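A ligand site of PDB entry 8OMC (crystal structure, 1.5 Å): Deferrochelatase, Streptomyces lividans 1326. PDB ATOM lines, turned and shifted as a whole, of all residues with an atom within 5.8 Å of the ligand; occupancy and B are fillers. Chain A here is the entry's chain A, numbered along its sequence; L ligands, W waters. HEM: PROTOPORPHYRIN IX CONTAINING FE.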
ATOM      1  N   ASN A 233      -6.964 -16.324  16.539  1.00  0.00           N
ATOM      2  CA  ASN A 233      -8.319 -16.614  17.018  1.00  0.00           C
ATOM      3  C   ASN A 233      -8.341 -16.688  18.550  1.00  0.00           C
ATOM      4  O   ASN A 233      -7.297 -16.522  19.198  1.00  0.00           O
ATOM      5  CB  ASN A 233      -8.928 -17.825  16.320  1.00  0.00           C
ATOM      6  CG  ASN A 233      -8.093 -19.073  16.576  1.00  0.00           C
ATOM      7  OD1 ASN A 233      -7.630 -19.293  17.710  1.00  0.00           O
ATOM      8  ND2 ASN A 233      -7.840 -19.876  15.558  1.00  0.00           N
ATOM      9  N   LEU A 235      -8.708 -19.157  20.471  1.00  0.00           N
ATOM     10  CA  LEU A 235      -7.956 -20.282  20.977  1.00  0.00           C
ATOM     11  C   LEU A 235      -6.471 -19.940  21.056  1.00  0.00           C
ATOM     12  O   LEU A 235      -5.689 -20.745  21.551  1.00  0.00           O
ATOM     13  CB  LEU A 235      -8.209 -21.535  20.125  1.00  0.00           C
ATOM     14  CG  LEU A 235      -9.670 -21.976  20.006  1.00  0.00           C
ATOM     15  CD1 LEU A 235      -9.758 -23.324  19.326  1.00  0.00           C
ATOM     16  CD2 LEU A 235     -10.387 -22.048  21.340  1.00  0.00           C
ATOM     17  N   PHE A 237      -4.282 -19.343  18.609  1.00  0.00           N
ATOM     18  CA  PHE A 237      -3.502 -19.750  17.436  1.00  0.00           C
ATOM     19  C   PHE A 237      -3.693 -18.767  16.289  1.00  0.00           C
ATOM     20  O   PHE A 237      -4.781 -18.238  16.029  1.00  0.00           O
ATOM     21  CB  PHE A 237      -3.896 -21.175  16.961  1.00  0.00           C
ATOM     22  CG  PHE A 237      -3.286 -22.274  17.790  1.00  0.00           C
ATOM     23  CD1 PHE A 237      -3.709 -22.535  19.082  1.00  0.00           C
ATOM     24  CD2 PHE A 237      -2.172 -22.977  17.338  1.00  0.00           C
ATOM     25  CE1 PHE A 237      -3.189 -23.562  19.842  1.00  0.00           C
ATOM     26  CE2 PHE A 237      -1.636 -23.997  18.089  1.00  0.00           C
ATOM     27  CZ  PHE A 237      -2.089 -24.277  19.359  1.00  0.00           C
ATOM     28  N   LYS A 238      -2.599 -18.533  15.547  1.00  0.00           N
ATOM     29  CA  LYS A 238      -2.635 -17.857  14.268  1.00  0.00           C
ATOM     30  C   LYS A 238      -3.561 -18.630  13.359  1.00  0.00           C
ATOM     31  O   LYS A 238      -3.529 -19.850  13.262  1.00  0.00           O
ATOM     32  CB  LYS A 238      -1.213 -17.903  13.677  1.00  0.00           C
ATOM     33  CG  LYS A 238      -0.206 -16.989  14.333  1.00  0.00           C
ATOM     34  CD  LYS A 238       1.197 -17.146  13.706  1.00  0.00           C
ATOM     35  CE  LYS A 238       2.249 -16.318  14.410  1.00  0.00           C
ATOM     36  NZ  LYS A 238       3.600 -16.492  13.767  1.00  0.00           N
ATOM     37  N   ASP A 239      -4.378 -17.886  12.638  1.00  0.00           N
ATOM     38  CA  ASP A 239      -5.420 -18.385  11.775  1.00  0.00           C
ATOM     39  C   ASP A 239      -5.361 -17.582  10.481  1.00  0.00           C
ATOM     40  O   ASP A 239      -5.666 -16.368  10.461  1.00  0.00           O
ATOM     41  CB  ASP A 239      -6.759 -18.306  12.526  1.00  0.00           C
ATOM     42  CG  ASP A 239      -7.861 -19.217  12.028  1.00  0.00           C
ATOM     43  OD1 ASP A 239      -7.795 -19.797  10.920  1.00  0.00           O
ATOM     44  OD2 ASP A 239      -8.791 -19.445  12.853  1.00  0.00           O
ATOM     45  N   GLY A 240      -4.973 -18.303   9.395  1.00  0.00           N
ATOM     46  CA  GLY A 240      -4.901 -17.752   8.048  1.00  0.00           C
ATOM     47  C   GLY A 240      -3.552 -17.884   7.353  1.00  0.00           C
ATOM     48  O   GLY A 240      -3.384 -17.303   6.269  1.00  0.00           O
ATOM     49  N   THR A 241      -2.626 -18.616   7.973  1.00  0.00           N
ATOM     50  CA  THR A 241      -1.306 -18.789   7.364  1.00  0.00           C
ATOM     51  C   THR A 241      -1.398 -19.360   5.946  1.00  0.00           C
ATOM     52  O   THR A 241      -0.802 -18.742   5.049  1.00  0.00           O
ATOM     53  CB  THR A 241      -0.505 -19.772   8.181  1.00  0.00           C
ATOM     54  OG1 THR A 241      -0.383 -19.255   9.503  1.00  0.00           O
ATOM     55  CG2 THR A 241       0.897 -19.981   7.656  1.00  0.00           C
ATOM     56  N   ARG A 242      -2.089 -20.479   5.743  1.00  0.00           N
ATOM     57  CA  ARG A 242      -2.197 -21.074   4.406  1.00  0.00           C
ATOM     58  C   ARG A 242      -3.599 -20.901   3.855  1.00  0.00           C
ATOM     59  O   ARG A 242      -4.440 -21.738   4.102  1.00  0.00           O
ATOM     60  CB  ARG A 242      -1.826 -22.540   4.459  1.00  0.00           C
ATOM     61  CG  ARG A 242      -0.298 -22.753   4.382  1.00  0.00           C
ATOM     62  CD  ARG A 242       0.143 -24.192   4.466  1.00  0.00           C
ATOM     63  NE  ARG A 242      -0.649 -25.127   3.688  1.00  0.00           N
ATOM     64  CZ  ARG A 242      -0.838 -25.072   2.355  1.00  0.00           C
ATOM     65  NH1 ARG A 242      -1.930 -25.619   1.806  1.00  0.00           N
ATOM     66  NH2 ARG A 242       0.092 -24.507   1.568  1.00  0.00           N
ATOM     67  N   ASN A 243      -3.839 -19.726   3.251  1.00  0.00           N
ATOM     68  CA  ASN A 243      -5.114 -19.328   2.710  1.00  0.00           C
ATOM     69  C   ASN A 243      -4.874 -19.108   1.215  1.00  0.00           C
ATOM     70  O   ASN A 243      -4.195 -19.892   0.571  1.00  0.00           O
ATOM     71  CB  ASN A 243      -5.665 -18.175   3.583  1.00  0.00           C
ATOM     72  CG  ASN A 243      -7.143 -17.953   3.337  1.00  0.00           C
ATOM     73  OD1 ASN A 243      -7.875 -18.947   3.268  1.00  0.00           O
ATOM     74  ND2 ASN A 243      -7.502 -16.670   3.221  1.00  0.00           N
ATOM     75  N   ARG A 276     -20.428 -20.000   8.817  1.00  0.00           N
ATOM     76  CA  ARG A 276     -20.734 -20.904   9.941  1.00  0.00           C
ATOM     77  C   ARG A 276     -20.408 -20.199  11.245  1.00  0.00           C
ATOM     78  O   ARG A 276     -19.278 -19.741  11.458  1.00  0.00           O
ATOM     79  CB  ARG A 276     -19.912 -22.198   9.832  1.00  0.00           C
ATOM     80  CG  ARG A 276     -20.049 -23.006   8.568  1.00  0.00           C
ATOM     81  CD  ARG A 276     -21.361 -23.771   8.520  1.00  0.00           C
ATOM     82  NE  ARG A 276     -21.330 -24.910   9.409  1.00  0.00           N
ATOM     83  CZ  ARG A 276     -22.183 -25.933   9.370  1.00  0.00           C
ATOM     84  NH1 ARG A 276     -23.202 -25.955   8.484  1.00  0.00           N
ATOM     85  NH2 ARG A 276     -21.908 -27.022  10.055  1.00  0.00           N
ATOM     86  N   ILE A 278     -19.487 -20.588  14.798  1.00  0.00           N
ATOM     87  CA  ILE A 278     -18.864 -21.680  15.531  1.00  0.00           C
ATOM     88  C   ILE A 278     -18.566 -21.259  16.980  1.00  0.00           C
ATOM     89  O   ILE A 278     -17.753 -20.382  17.253  1.00  0.00           O
ATOM     90  CB  ILE A 278     -17.617 -22.205  14.796  1.00  0.00           C
ATOM     91  CG1 ILE A 278     -17.900 -22.564  13.338  1.00  0.00           C
ATOM     92  CG2 ILE A 278     -17.138 -23.412  15.596  1.00  0.00           C
ATOM     93  CD1 ILE A 278     -16.623 -22.906  12.547  1.00  0.00           C
ATOM     94  N   MET A 280     -17.038 -21.640  20.596  1.00  0.00           N
ATOM     95  CA  MET A 280     -15.851 -22.293  21.145  1.00  0.00           C
ATOM     96  C   MET A 280     -16.114 -22.687  22.591  1.00  0.00           C
ATOM     97  O   MET A 280     -16.584 -21.872  23.392  1.00  0.00           O
ATOM     98  CB  MET A 280     -14.644 -21.348  21.122  1.00  0.00           C
ATOM     99  CG  MET A 280     -14.070 -21.226  19.740  1.00  0.00           C
ATOM    100  SD  MET A 280     -12.965 -19.769  19.643  1.00  0.00           S
ATOM    101  CE  MET A 280     -12.239 -20.039  18.037  1.00  0.00           C
ATOM    102  N   PHE A 297      -4.093 -28.924  16.438  1.00  0.00           N
ATOM    103  CA  PHE A 297      -3.920 -28.181  15.199  1.00  0.00           C
ATOM    104  C   PHE A 297      -2.873 -28.844  14.301  1.00  0.00           C
ATOM    105  O   PHE A 297      -3.047 -28.822  13.088  1.00  0.00           O
ATOM    106  CB  PHE A 297      -3.608 -26.714  15.491  1.00  0.00           C
ATOM    107  CG  PHE A 297      -4.887 -25.993  15.854  1.00  0.00           C
ATOM    108  CD1 PHE A 297      -5.913 -25.885  14.915  1.00  0.00           C
ATOM    109  CD2 PHE A 297      -5.029 -25.481  17.115  1.00  0.00           C
ATOM    110  CE1 PHE A 297      -7.118 -25.296  15.294  1.00  0.00           C
ATOM    111  CE2 PHE A 297      -6.197 -24.849  17.464  1.00  0.00           C
ATOM    112  CZ  PHE A 297      -7.238 -24.807  16.572  1.00  0.00           C
ATOM    113  N   ARG A 299       0.289 -27.486  14.597  1.00  0.00           N
ATOM    114  CA  ARG A 299       1.220 -26.381  14.560  1.00  0.00           C
ATOM    115  C   ARG A 299       1.516 -26.067  16.024  1.00  0.00           C
ATOM    116  O   ARG A 299       0.699 -26.341  16.894  1.00  0.00           O
ATOM    117  CB  ARG A 299       0.656 -25.159  13.838  1.00  0.00           C
ATOM    118  CG  ARG A 299       0.590 -25.324  12.328  1.00  0.00           C
ATOM    119  CD  ARG A 299      -0.084 -24.167  11.646  1.00  0.00           C
ATOM    120  NE  ARG A 299      -0.138 -24.239  10.187  1.00  0.00           N
ATOM    121  CZ  ARG A 299       0.841 -23.805   9.373  1.00  0.00           C
ATOM    122  NH1 ARG A 299       1.981 -23.301   9.865  1.00  0.00           N
ATOM    123  NH2 ARG A 299       0.655 -23.898   8.055  1.00  0.00           N
ATOM    124  N   PRO A 316       3.900 -27.439   5.754  1.00  0.00           N
ATOM    125  CA  PRO A 316       3.546 -28.585   6.570  1.00  0.00           C
ATOM    126  C   PRO A 316       4.138 -29.866   6.015  1.00  0.00           C
ATOM    127  O   PRO A 316       4.147 -30.083   4.791  1.00  0.00           O
ATOM    128  CB  PRO A 316       2.018 -28.622   6.390  1.00  0.00           C
ATOM    129  CG  PRO A 316       1.632 -27.281   6.030  1.00  0.00           C
ATOM    130  CD  PRO A 316       2.745 -26.689   5.230  1.00  0.00           C
ATOM    131  N   HIS A 326      -6.250 -30.873  12.905  1.00  0.00           N
ATOM    132  CA  HIS A 326      -7.061 -30.010  12.080  1.00  0.00           C
ATOM    133  C   HIS A 326      -6.362 -29.738  10.729  1.00  0.00           C
ATOM    134  O   HIS A 326      -6.972 -29.810   9.686  1.00  0.00           O
ATOM    135  CB  HIS A 326      -7.329 -28.684  12.825  1.00  0.00           C
ATOM    136  CG  HIS A 326      -8.175 -27.680  12.095  1.00  0.00           C
ATOM    137  ND1 HIS A 326      -9.529 -27.916  11.857  1.00  0.00           N
ATOM    138  CD2 HIS A 326      -7.888 -26.478  11.542  1.00  0.00           C
ATOM    139  CE1 HIS A 326      -9.993 -26.894  11.142  1.00  0.00           C
ATOM    140  NE2 HIS A 326      -9.042 -25.948  10.992  1.00  0.00           N
ATOM    141  N   VAL A 327      -5.085 -29.291  10.781  1.00  0.00           N
ATOM    142  CA  VAL A 327      -4.386 -28.874   9.564  1.00  0.00           C
ATOM    143  C   VAL A 327      -4.254 -30.095   8.640  1.00  0.00           C
ATOM    144  O   VAL A 327      -4.385 -29.962   7.421  1.00  0.00           O
ATOM    145  CB  VAL A 327      -3.017 -28.227   9.859  1.00  0.00           C
ATOM    146  CG1 VAL A 327      -2.191 -28.061   8.631  1.00  0.00           C
ATOM    147  CG2 VAL A 327      -3.211 -26.901  10.538  1.00  0.00           C
ATOM    148  N   ALA A 330      -7.641 -30.663   7.053  1.00  0.00           N
ATOM    149  CA  ALA A 330      -8.160 -29.560   6.271  1.00  0.00           C
ATOM    150  C   ALA A 330      -7.368 -29.309   4.973  1.00  0.00           C
ATOM    151  O   ALA A 330      -7.783 -28.575   4.071  1.00  0.00           O
ATOM    152  CB  ALA A 330      -8.277 -28.300   7.105  1.00  0.00           C
ATOM    153  N   HIS A 331      -6.071 -29.722   4.981  1.00  0.00           N
ATOM    154  CA  HIS A 331      -5.136 -29.328   3.964  1.00  0.00           C
ATOM    155  C   HIS A 331      -5.649 -29.824   2.604  1.00  0.00           C
ATOM    156  O   HIS A 331      -6.244 -30.905   2.504  1.00  0.00           O
ATOM    157  CB  HIS A 331      -3.783 -29.961   4.283  1.00  0.00           C
ATOM    158  CG  HIS A 331      -2.609 -29.432   3.512  1.00  0.00           C
ATOM    159  ND1 HIS A 331      -2.439 -29.792   2.190  1.00  0.00           N
ATOM    160  CD2 HIS A 331      -1.562 -28.660   3.856  1.00  0.00           C
ATOM    161  CE1 HIS A 331      -1.357 -29.193   1.715  1.00  0.00           C
ATOM    162  NE2 HIS A 331      -0.741 -28.472   2.761  1.00  0.00           N
ATOM    163  N   PRO A 332      -5.452 -29.013   1.539  1.00  0.00           N
ATOM    164  CA  PRO A 332      -5.887 -29.463   0.195  1.00  0.00           C
ATOM    165  C   PRO A 332      -5.365 -30.824  -0.227  1.00  0.00           C
ATOM    166  O   PRO A 332      -6.117 -31.584  -0.844  1.00  0.00           O
ATOM    167  CB  PRO A 332      -5.285 -28.339  -0.667  1.00  0.00           C
ATOM    168  CG  PRO A 332      -5.400 -27.117   0.182  1.00  0.00           C
ATOM    169  CD  PRO A 332      -4.981 -27.622   1.535  1.00  0.00           C
ATOM    170  N   LEU A 340      -9.818 -23.301  -0.046  1.00  0.00           N
ATOM    171  CA  LEU A 340     -10.757 -22.276   0.364  1.00  0.00           C
ATOM    172  C   LEU A 340     -10.070 -20.922   0.497  1.00  0.00           C
ATOM    173  O   LEU A 340      -8.856 -20.888   0.803  1.00  0.00           O
ATOM    174  CB  LEU A 340     -11.300 -22.669   1.750  1.00  0.00           C
ATOM    175  CG  LEU A 340     -11.905 -24.061   1.926  1.00  0.00           C
ATOM    176  CD1 LEU A 340     -12.457 -24.251   3.352  1.00  0.00           C
ATOM    177  CD2 LEU A 340     -13.011 -24.340   0.945  1.00  0.00           C
ATOM    178  N   ARG A 342     -10.582 -18.505   3.261  1.00  0.00           N
ATOM    179  CA  ARG A 342     -11.180 -18.251   4.568  1.00  0.00           C
ATOM    180  C   ARG A 342     -11.046 -16.776   4.929  1.00  0.00           C
ATOM    181  O   ARG A 342     -10.020 -16.163   4.661  1.00  0.00           O
ATOM    182  CB  ARG A 342     -10.529 -19.094   5.664  1.00  0.00           C
ATOM    183  CG  ARG A 342     -10.708 -20.593   5.419  1.00  0.00           C
ATOM    184  CD  ARG A 342      -9.879 -21.448   6.320  1.00  0.00           C
ATOM    185  NE  ARG A 342      -8.467 -21.381   5.963  1.00  0.00           N
ATOM    186  CZ  ARG A 342      -7.444 -21.189   6.783  1.00  0.00           C
ATOM    187  NH1 ARG A 342      -7.550 -21.012   8.106  1.00  0.00           N
ATOM    188  NH2 ARG A 342      -6.239 -21.132   6.248  1.00  0.00           N
ATOM    189  N   LEU A 361     -16.079 -18.152  16.767  1.00  0.00           N
ATOM    190  CA  LEU A 361     -15.530 -17.711  15.512  1.00  0.00           C
ATOM    191  C   LEU A 361     -16.638 -17.793  14.477  1.00  0.00           C
ATOM    192  O   LEU A 361     -17.324 -18.791  14.335  1.00  0.00           O
ATOM    193  CB  LEU A 361     -14.317 -18.614  15.207  1.00  0.00           C
ATOM    194  CG  LEU A 361     -13.397 -18.146  14.079  1.00  0.00           C
ATOM    195  CD1 LEU A 361     -12.023 -18.720  14.233  1.00  0.00           C
ATOM    196  CD2 LEU A 361     -13.931 -18.562  12.727  1.00  0.00           C
ATOM    197  N   PHE A 363     -17.050 -18.134  10.930  1.00  0.00           N
ATOM    198  CA  PHE A 363     -16.234 -18.710   9.869  1.00  0.00           C
ATOM    199  C   PHE A 363     -16.898 -18.358   8.533  1.00  0.00           C
ATOM    200  O   PHE A 363     -18.103 -18.466   8.391  1.00  0.00           O
ATOM    201  CB  PHE A 363     -16.184 -20.237  10.054  1.00  0.00           C
ATOM    202  CG  PHE A 363     -15.412 -20.920   8.962  1.00  0.00           C
ATOM    203  CD1 PHE A 363     -16.029 -21.311   7.802  1.00  0.00           C
ATOM    204  CD2 PHE A 363     -14.057 -21.158   9.118  1.00  0.00           C
ATOM    205  CE1 PHE A 363     -15.328 -22.007   6.810  1.00  0.00           C
ATOM    206  CE2 PHE A 363     -13.344 -21.812   8.139  1.00  0.00           C
ATOM    207  CZ  PHE A 363     -13.988 -22.235   6.991  1.00  0.00           C
ATOM    208  N   PHE A 374     -16.062 -26.115   0.462  1.00  0.00           N
ATOM    209  CA  PHE A 374     -16.383 -26.324   1.879  1.00  0.00           C
ATOM    210  C   PHE A 374     -16.856 -27.740   2.167  1.00  0.00           C
ATOM    211  O   PHE A 374     -16.497 -28.353   3.175  1.00  0.00           O
ATOM    212  CB  PHE A 374     -17.418 -25.291   2.324  1.00  0.00           C
ATOM    213  CG  PHE A 374     -17.902 -25.467   3.728  1.00  0.00           C
ATOM    214  CD1 PHE A 374     -17.199 -24.863   4.761  1.00  0.00           C
ATOM    215  CD2 PHE A 374     -18.998 -26.259   4.070  1.00  0.00           C
ATOM    216  CE1 PHE A 374     -17.535 -25.114   6.079  1.00  0.00           C
ATOM    217  CE2 PHE A 374     -19.386 -26.426   5.369  1.00  0.00           C
ATOM    218  CZ  PHE A 374     -18.679 -25.825   6.385  1.00  0.00           C
ATOM    219  N   VAL A 377     -14.133 -30.484   2.461  1.00  0.00           N
ATOM    220  CA  VAL A 377     -13.245 -30.165   3.571  1.00  0.00           C
ATOM    221  C   VAL A 377     -13.981 -30.417   4.878  1.00  0.00           C
ATOM    222  O   VAL A 377     -13.484 -31.084   5.799  1.00  0.00           O
ATOM    223  CB  VAL A 377     -12.645 -28.759   3.440  1.00  0.00           C
ATOM    224  CG1 VAL A 377     -11.719 -28.428   4.601  1.00  0.00           C
ATOM    225  CG2 VAL A 377     -11.828 -28.610   2.164  1.00  0.00           C
ATOM    226  N   GLN A 378     -15.193 -29.900   5.046  1.00  0.00           N
ATOM    227  CA  GLN A 378     -15.894 -30.071   6.307  1.00  0.00           C
ATOM    228  C   GLN A 378     -16.213 -31.551   6.570  1.00  0.00           C
ATOM    229  O   GLN A 378     -16.131 -32.043   7.718  1.00  0.00           O
ATOM    230  CB  GLN A 378     -17.136 -29.162   6.384  1.00  0.00           C
ATOM    231  CG  GLN A 378     -17.968 -29.344   7.651  1.00  0.00           C
ATOM    232  CD  GLN A 378     -17.271 -28.953   8.941  1.00  0.00           C
ATOM    233  OE1 GLN A 378     -16.473 -28.034   8.933  1.00  0.00           O
ATOM    234  NE2 GLN A 378     -17.688 -29.472  10.082  1.00  0.00           N
ATOM    235  N   LEU A 381     -13.418 -33.112   8.171  1.00  0.00           N
ATOM    236  CA  LEU A 381     -13.242 -32.749   9.582  1.00  0.00           C
ATOM    237  C   LEU A 381     -14.133 -33.549  10.538  1.00  0.00           C
ATOM    238  O   LEU A 381     -14.150 -33.292  11.739  1.00  0.00           O
ATOM    239  CB  LEU A 381     -13.454 -31.245   9.774  1.00  0.00           C
ATOM    240  CG  LEU A 381     -12.579 -30.308   8.960  1.00  0.00           C
ATOM    241  CD1 LEU A 381     -12.876 -28.820   9.310  1.00  0.00           C
ATOM    242  CD2 LEU A 381     -11.099 -30.602   9.112  1.00  0.00           C
ATOM    243  N   LEU A 386     -10.237 -30.981  16.793  1.00  0.00           N
ATOM    244  CA  LEU A 386     -10.830 -29.706  17.197  1.00  0.00           C
ATOM    245  C   LEU A 386     -12.321 -29.894  17.559  1.00  0.00           C
ATOM    246  O   LEU A 386     -12.873 -29.059  18.261  1.00  0.00           O
ATOM    247  CB  LEU A 386     -10.618 -28.699  16.064  1.00  0.00           C
ATOM    248  CG  LEU A 386     -11.149 -27.271  16.257  1.00  0.00           C
ATOM    249  CD1 LEU A 386     -10.426 -26.587  17.406  1.00  0.00           C
ATOM    250  CD2 LEU A 386     -11.009 -26.497  14.947  1.00  0.00           C
ATOM    251  N   ILE A 390     -15.440 -27.202  19.853  1.00  0.00           N
ATOM    252  CA  ILE A 390     -16.274 -26.298  19.105  1.00  0.00           C
ATOM    253  C   ILE A 390     -17.648 -26.946  18.863  1.00  0.00           C
ATOM    254  O   ILE A 390     -17.836 -28.161  18.927  1.00  0.00           O
ATOM    255  CB  ILE A 390     -15.628 -25.932  17.763  1.00  0.00           C
ATOM    256  CG1 ILE A 390     -15.474 -27.162  16.846  1.00  0.00           C
ATOM    257  CG2 ILE A 390     -14.313 -25.200  17.953  1.00  0.00           C
ATOM    258  CD1 ILE A 390     -15.127 -26.865  15.418  1.00  0.00           C
ATOM    259  N   HIS A 392     -20.740 -26.041  15.797  1.00  0.00           N
ATOM    260  CA  HIS A 392     -21.385 -25.191  14.799  1.00  0.00           C
ATOM    261  C   HIS A 392     -22.872 -24.962  15.140  1.00  0.00           C
ATOM    262  O   HIS A 392     -23.613 -25.940  15.357  1.00  0.00           O
ATOM    263  CB  HIS A 392     -21.316 -25.830  13.425  1.00  0.00           C
ATOM    264  CG  HIS A 392     -19.937 -26.017  12.858  1.00  0.00           C
ATOM    265  ND1 HIS A 392     -19.618 -25.541  11.628  1.00  0.00           N
ATOM    266  CD2 HIS A 392     -18.824 -26.634  13.356  1.00  0.00           C
ATOM    267  CE1 HIS A 392     -18.359 -25.863  11.358  1.00  0.00           C
ATOM    268  NE2 HIS A 392     -17.832 -26.514  12.424  1.00  0.00           N
HETATM  269  CHA HEM L   1      -6.043 -23.937   9.129  1.00  0.00           C
HETATM  270  CHB HEM L   1      -8.174 -22.850  13.334  1.00  0.00           C
HETATM  271  CHC HEM L   1     -12.572 -24.010  11.417  1.00  0.00           C
HETATM  272  CHD HEM L   1     -10.441 -25.013   7.194  1.00  0.00           C
HETATM  273  C1A HEM L   1      -6.219 -23.535  10.453  1.00  0.00           C
HETATM  274  C2A HEM L   1      -5.253 -23.128  11.389  1.00  0.00           C
HETATM  275  C3A HEM L   1      -5.838 -22.822  12.573  1.00  0.00           C
HETATM  276  C4A HEM L   1      -7.228 -23.015  12.371  1.00  0.00           C
HETATM  277  CMA HEM L   1      -5.234 -22.372  13.881  1.00  0.00           C
HETATM  278  CAA HEM L   1      -3.759 -23.088  11.041  1.00  0.00           C
HETATM  279  CBA HEM L   1      -3.198 -21.854  10.321  1.00  0.00           C
HETATM  280  CGA HEM L   1      -3.743 -21.645   8.943  1.00  0.00           C
HETATM  281  O1A HEM L   1      -4.769 -20.941   8.778  1.00  0.00           O
HETATM  282  O2A HEM L   1      -3.084 -22.139   8.001  1.00  0.00           O
HETATM  283  C1B HEM L   1      -9.556 -23.028  13.179  1.00  0.00           C
HETATM  284  C2B HEM L   1     -10.568 -22.818  14.213  1.00  0.00           C
HETATM  285  C3B HEM L   1     -11.788 -23.184  13.659  1.00  0.00           C
HETATM  286  C4B HEM L   1     -11.565 -23.649  12.300  1.00  0.00           C
HETATM  287  CMB HEM L   1     -10.237 -22.274  15.564  1.00  0.00           C
HETATM  288  CAB HEM L   1     -13.180 -23.083  14.240  1.00  0.00           C
HETATM  289  CBB HEM L   1     -13.458 -22.382  15.304  1.00  0.00           C
HETATM  290  C1C HEM L   1     -12.431 -24.424  10.128  1.00  0.00           C
HETATM  291  C2C HEM L   1     -13.375 -24.895   9.200  1.00  0.00           C
HETATM  292  C3C HEM L   1     -12.741 -25.179   8.072  1.00  0.00           C
HETATM  293  C4C HEM L   1     -11.358 -24.868   8.168  1.00  0.00           C
HETATM  294  CMC HEM L   1     -14.826 -24.995   9.528  1.00  0.00           C
HETATM  295  CAC HEM L   1     -13.309 -25.723   6.830  1.00  0.00           C
HETATM  296  CBC HEM L   1     -14.432 -26.414   6.736  1.00  0.00           C
HETATM  297  C1D HEM L   1      -9.048 -24.743   7.398  1.00  0.00           C
HETATM  298  C2D HEM L   1      -8.081 -24.794   6.271  1.00  0.00           C
HETATM  299  C3D HEM L   1      -6.837 -24.626   6.812  1.00  0.00           C
HETATM  300  C4D HEM L   1      -7.106 -24.268   8.219  1.00  0.00           C
HETATM  301  CMD HEM L   1      -8.420 -25.178   4.847  1.00  0.00           C
HETATM  302  CAD HEM L   1      -5.448 -24.538   6.086  1.00  0.00           C
HETATM  303  CBD HEM L   1      -4.942 -25.960   6.001  1.00  0.00           C
HETATM  304  CGD HEM L   1      -3.658 -25.997   5.111  1.00  0.00           C
HETATM  305  O1D HEM L   1      -2.535 -25.931   5.642  1.00  0.00           O
HETATM  306  O2D HEM L   1      -3.859 -25.904   3.871  1.00  0.00           O
HETATM  307  NA  HEM L   1      -7.440 -23.496  11.097  1.00  0.00           N
HETATM  308  NB  HEM L   1     -10.197 -23.507  12.117  1.00  0.00           N
HETATM  309  NC  HEM L   1     -11.152 -24.419   9.489  1.00  0.00           N
HETATM  310  ND  HEM L   1      -8.400 -24.379   8.505  1.00  0.00           N
HETATM  311 FE   HEM L   1      -9.278 -24.038  10.312  1.00  0.00          FE
HETATM  312  O   HOH W   1      -5.013 -23.996   2.400  1.00  0.00           O
HETATM  313  O   HOH W   2      -7.625 -24.353   1.717  1.00  0.00           O
HETATM  314  O   HOH W   3      -9.513 -21.824   9.952  1.00  0.00           O
HETATM  315  O   HOH W   4     -11.002 -20.440  11.684  1.00  0.00           O
HETATM  316  O   HOH W   5      -2.021 -24.693   7.935  1.00  0.00           O
HETATM  317  O   HOH W   6      -8.566 -26.872   2.034  1.00  0.00           O
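An oxygen (O1A) of the ligand lies within salt-bridge range of the guanidinium group (NH1) of Arg 342 (2.9 Å). N of Arg 242 sits at hydrogen-bond distance from O2A of the ligand (3.0 Å). An iron atom (FE) of the ligand is bound by a ring nitrogen (NE2) of His 326, 2.0 Å away. An oxygen (O1A) of the ligand lies within hydrogen-bond range of the backbone NH (N) of Thr 241 (3.3 Å). An oxygen (O1A) of the ligand lies within hydrogen-bond range of the backbone NH (N) of Gly 240 (2.7 Å). An oxygen (O1D) of the ligand lies within salt-bridge range of the guanidinium group (NE) of Arg 242.
The guanidinium group (NH1) of Arg 242 lies within hydrogen-bond range of a ring nitrogen (NE2) of His 331 (3.2 Å). ND2 of Asn 233 is in hydrogen-bond range of OD2 of Asp 239, 2.9 Å away. The backbone NH (N) of Phe 237 is in hydrogen-bond range of the side-chain amide oxygen (OD1) of Asn 233, at 3.5 Å. The backbone carbonyl oxygen (O) of Phe 297 sits at hydrogen-bond distance from the backbone NH (N) of Val 327 (3.1 Å). O of Leu 340 sits close to OD1 of Asn 243 (3.3 Å). The backbone carbonyl oxygen (O) of Arg 276 sits at hydrogen-bond distance from the backbone NH (N) of Phe 363, at 2.8 Å. The backbone carbonyl oxygen of Arg 242 lies within hydrogen-bond range of the guanidinium group of Arg 342 (2.9 Å). OD1 of Asn 233 lies within hydrogen-bond range of N of Leu 235.
ND2 of Asn 233 touches CMB of the ligand, at 3.4 Å. Leu 235 touches the ligand (CD1 to CMB, 3.9 Å). CB of Phe 237 touches CMA of the ligand, 3.6 Å away. O of Lys 238 touches CMA of the ligand, at 3.1 Å. Asp 239 touches the ligand. CG2 of Ile 278 touches CBB of the ligand, 3.8 Å away. Met 280 touches the ligand (CE to CBB, 3.8 Å). CE1 of Phe 297 touches CHB of the ligand (3.3 Å). CD of Arg 299 touches CAA of the ligand (3.9 Å). Val 327 touches the ligand (CG1 to O1D, 3.7 Å). Ala 330 touches the ligand (O to CMD, 3.5 Å). His 331 touches the ligand (CD2 to O1D, 3.4 Å). Pro 332 touches the ligand (CD to O2D, 3.1 Å). CD1 of Leu 340 touches CAC of the ligand, at 3.9 Å. Leu 361 touches the ligand. Phe 363 touches the ligand. Phe 374 touches the ligand (CE1 to CBC, 3.4 Å). CG1 of Val 377 touches CAC of the ligand, at 3.8 Å. OE1 of Gln 378 touches CBC of the ligand, at 3.4 Å. Leu 381 touches the ligand (CD1 to C3C, 3.8 Å). Leu 386 touches the ligand (CD2 to C3B, 3.6 Å). Ile 390 touches the ligand. Hydrophobic or aromatic side chains within 4 Å of the ligand: Leu 235, Phe 237, Ile 278, Met 280, Phe 297, His 326, Val 327, Ala 330, His 331, Pro 332, Leu 340, Leu 361, Phe 363, Phe 374, Val 377, Leu 381, Leu 386 and Ile 390. Within 4 Å of the ligand: Asn 233, Leu 235, Phe 237, Lys 238, Asp 239, Gly 240, Thr 241, Arg 242, Ile 278, Met 280, Phe 297, Arg 299, His 326, Val 327, Ala 330, His 331, Pro 332, Leu 340, Arg 342, Leu 361, Phe 363, Phe 374, Val 377, Gln 378, Leu 381, Leu 386 and Ile 390. The nearest printed residue that does not touch the ligand is His 392 (4.1 Å).
Water W3 lies within hydrogen-bond range of the guanidinium group (NH1) of Arg 342 and the side-chain carboxylate (OD1) of Asp 239. Water W5 bridges O1D of the ligand (2.7 Å) and NH2 of Arg 299 (2.8 Å). Water W1 bridges O2D of the ligand (2.7 Å) and O of Arg 242 (2.9 Å).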
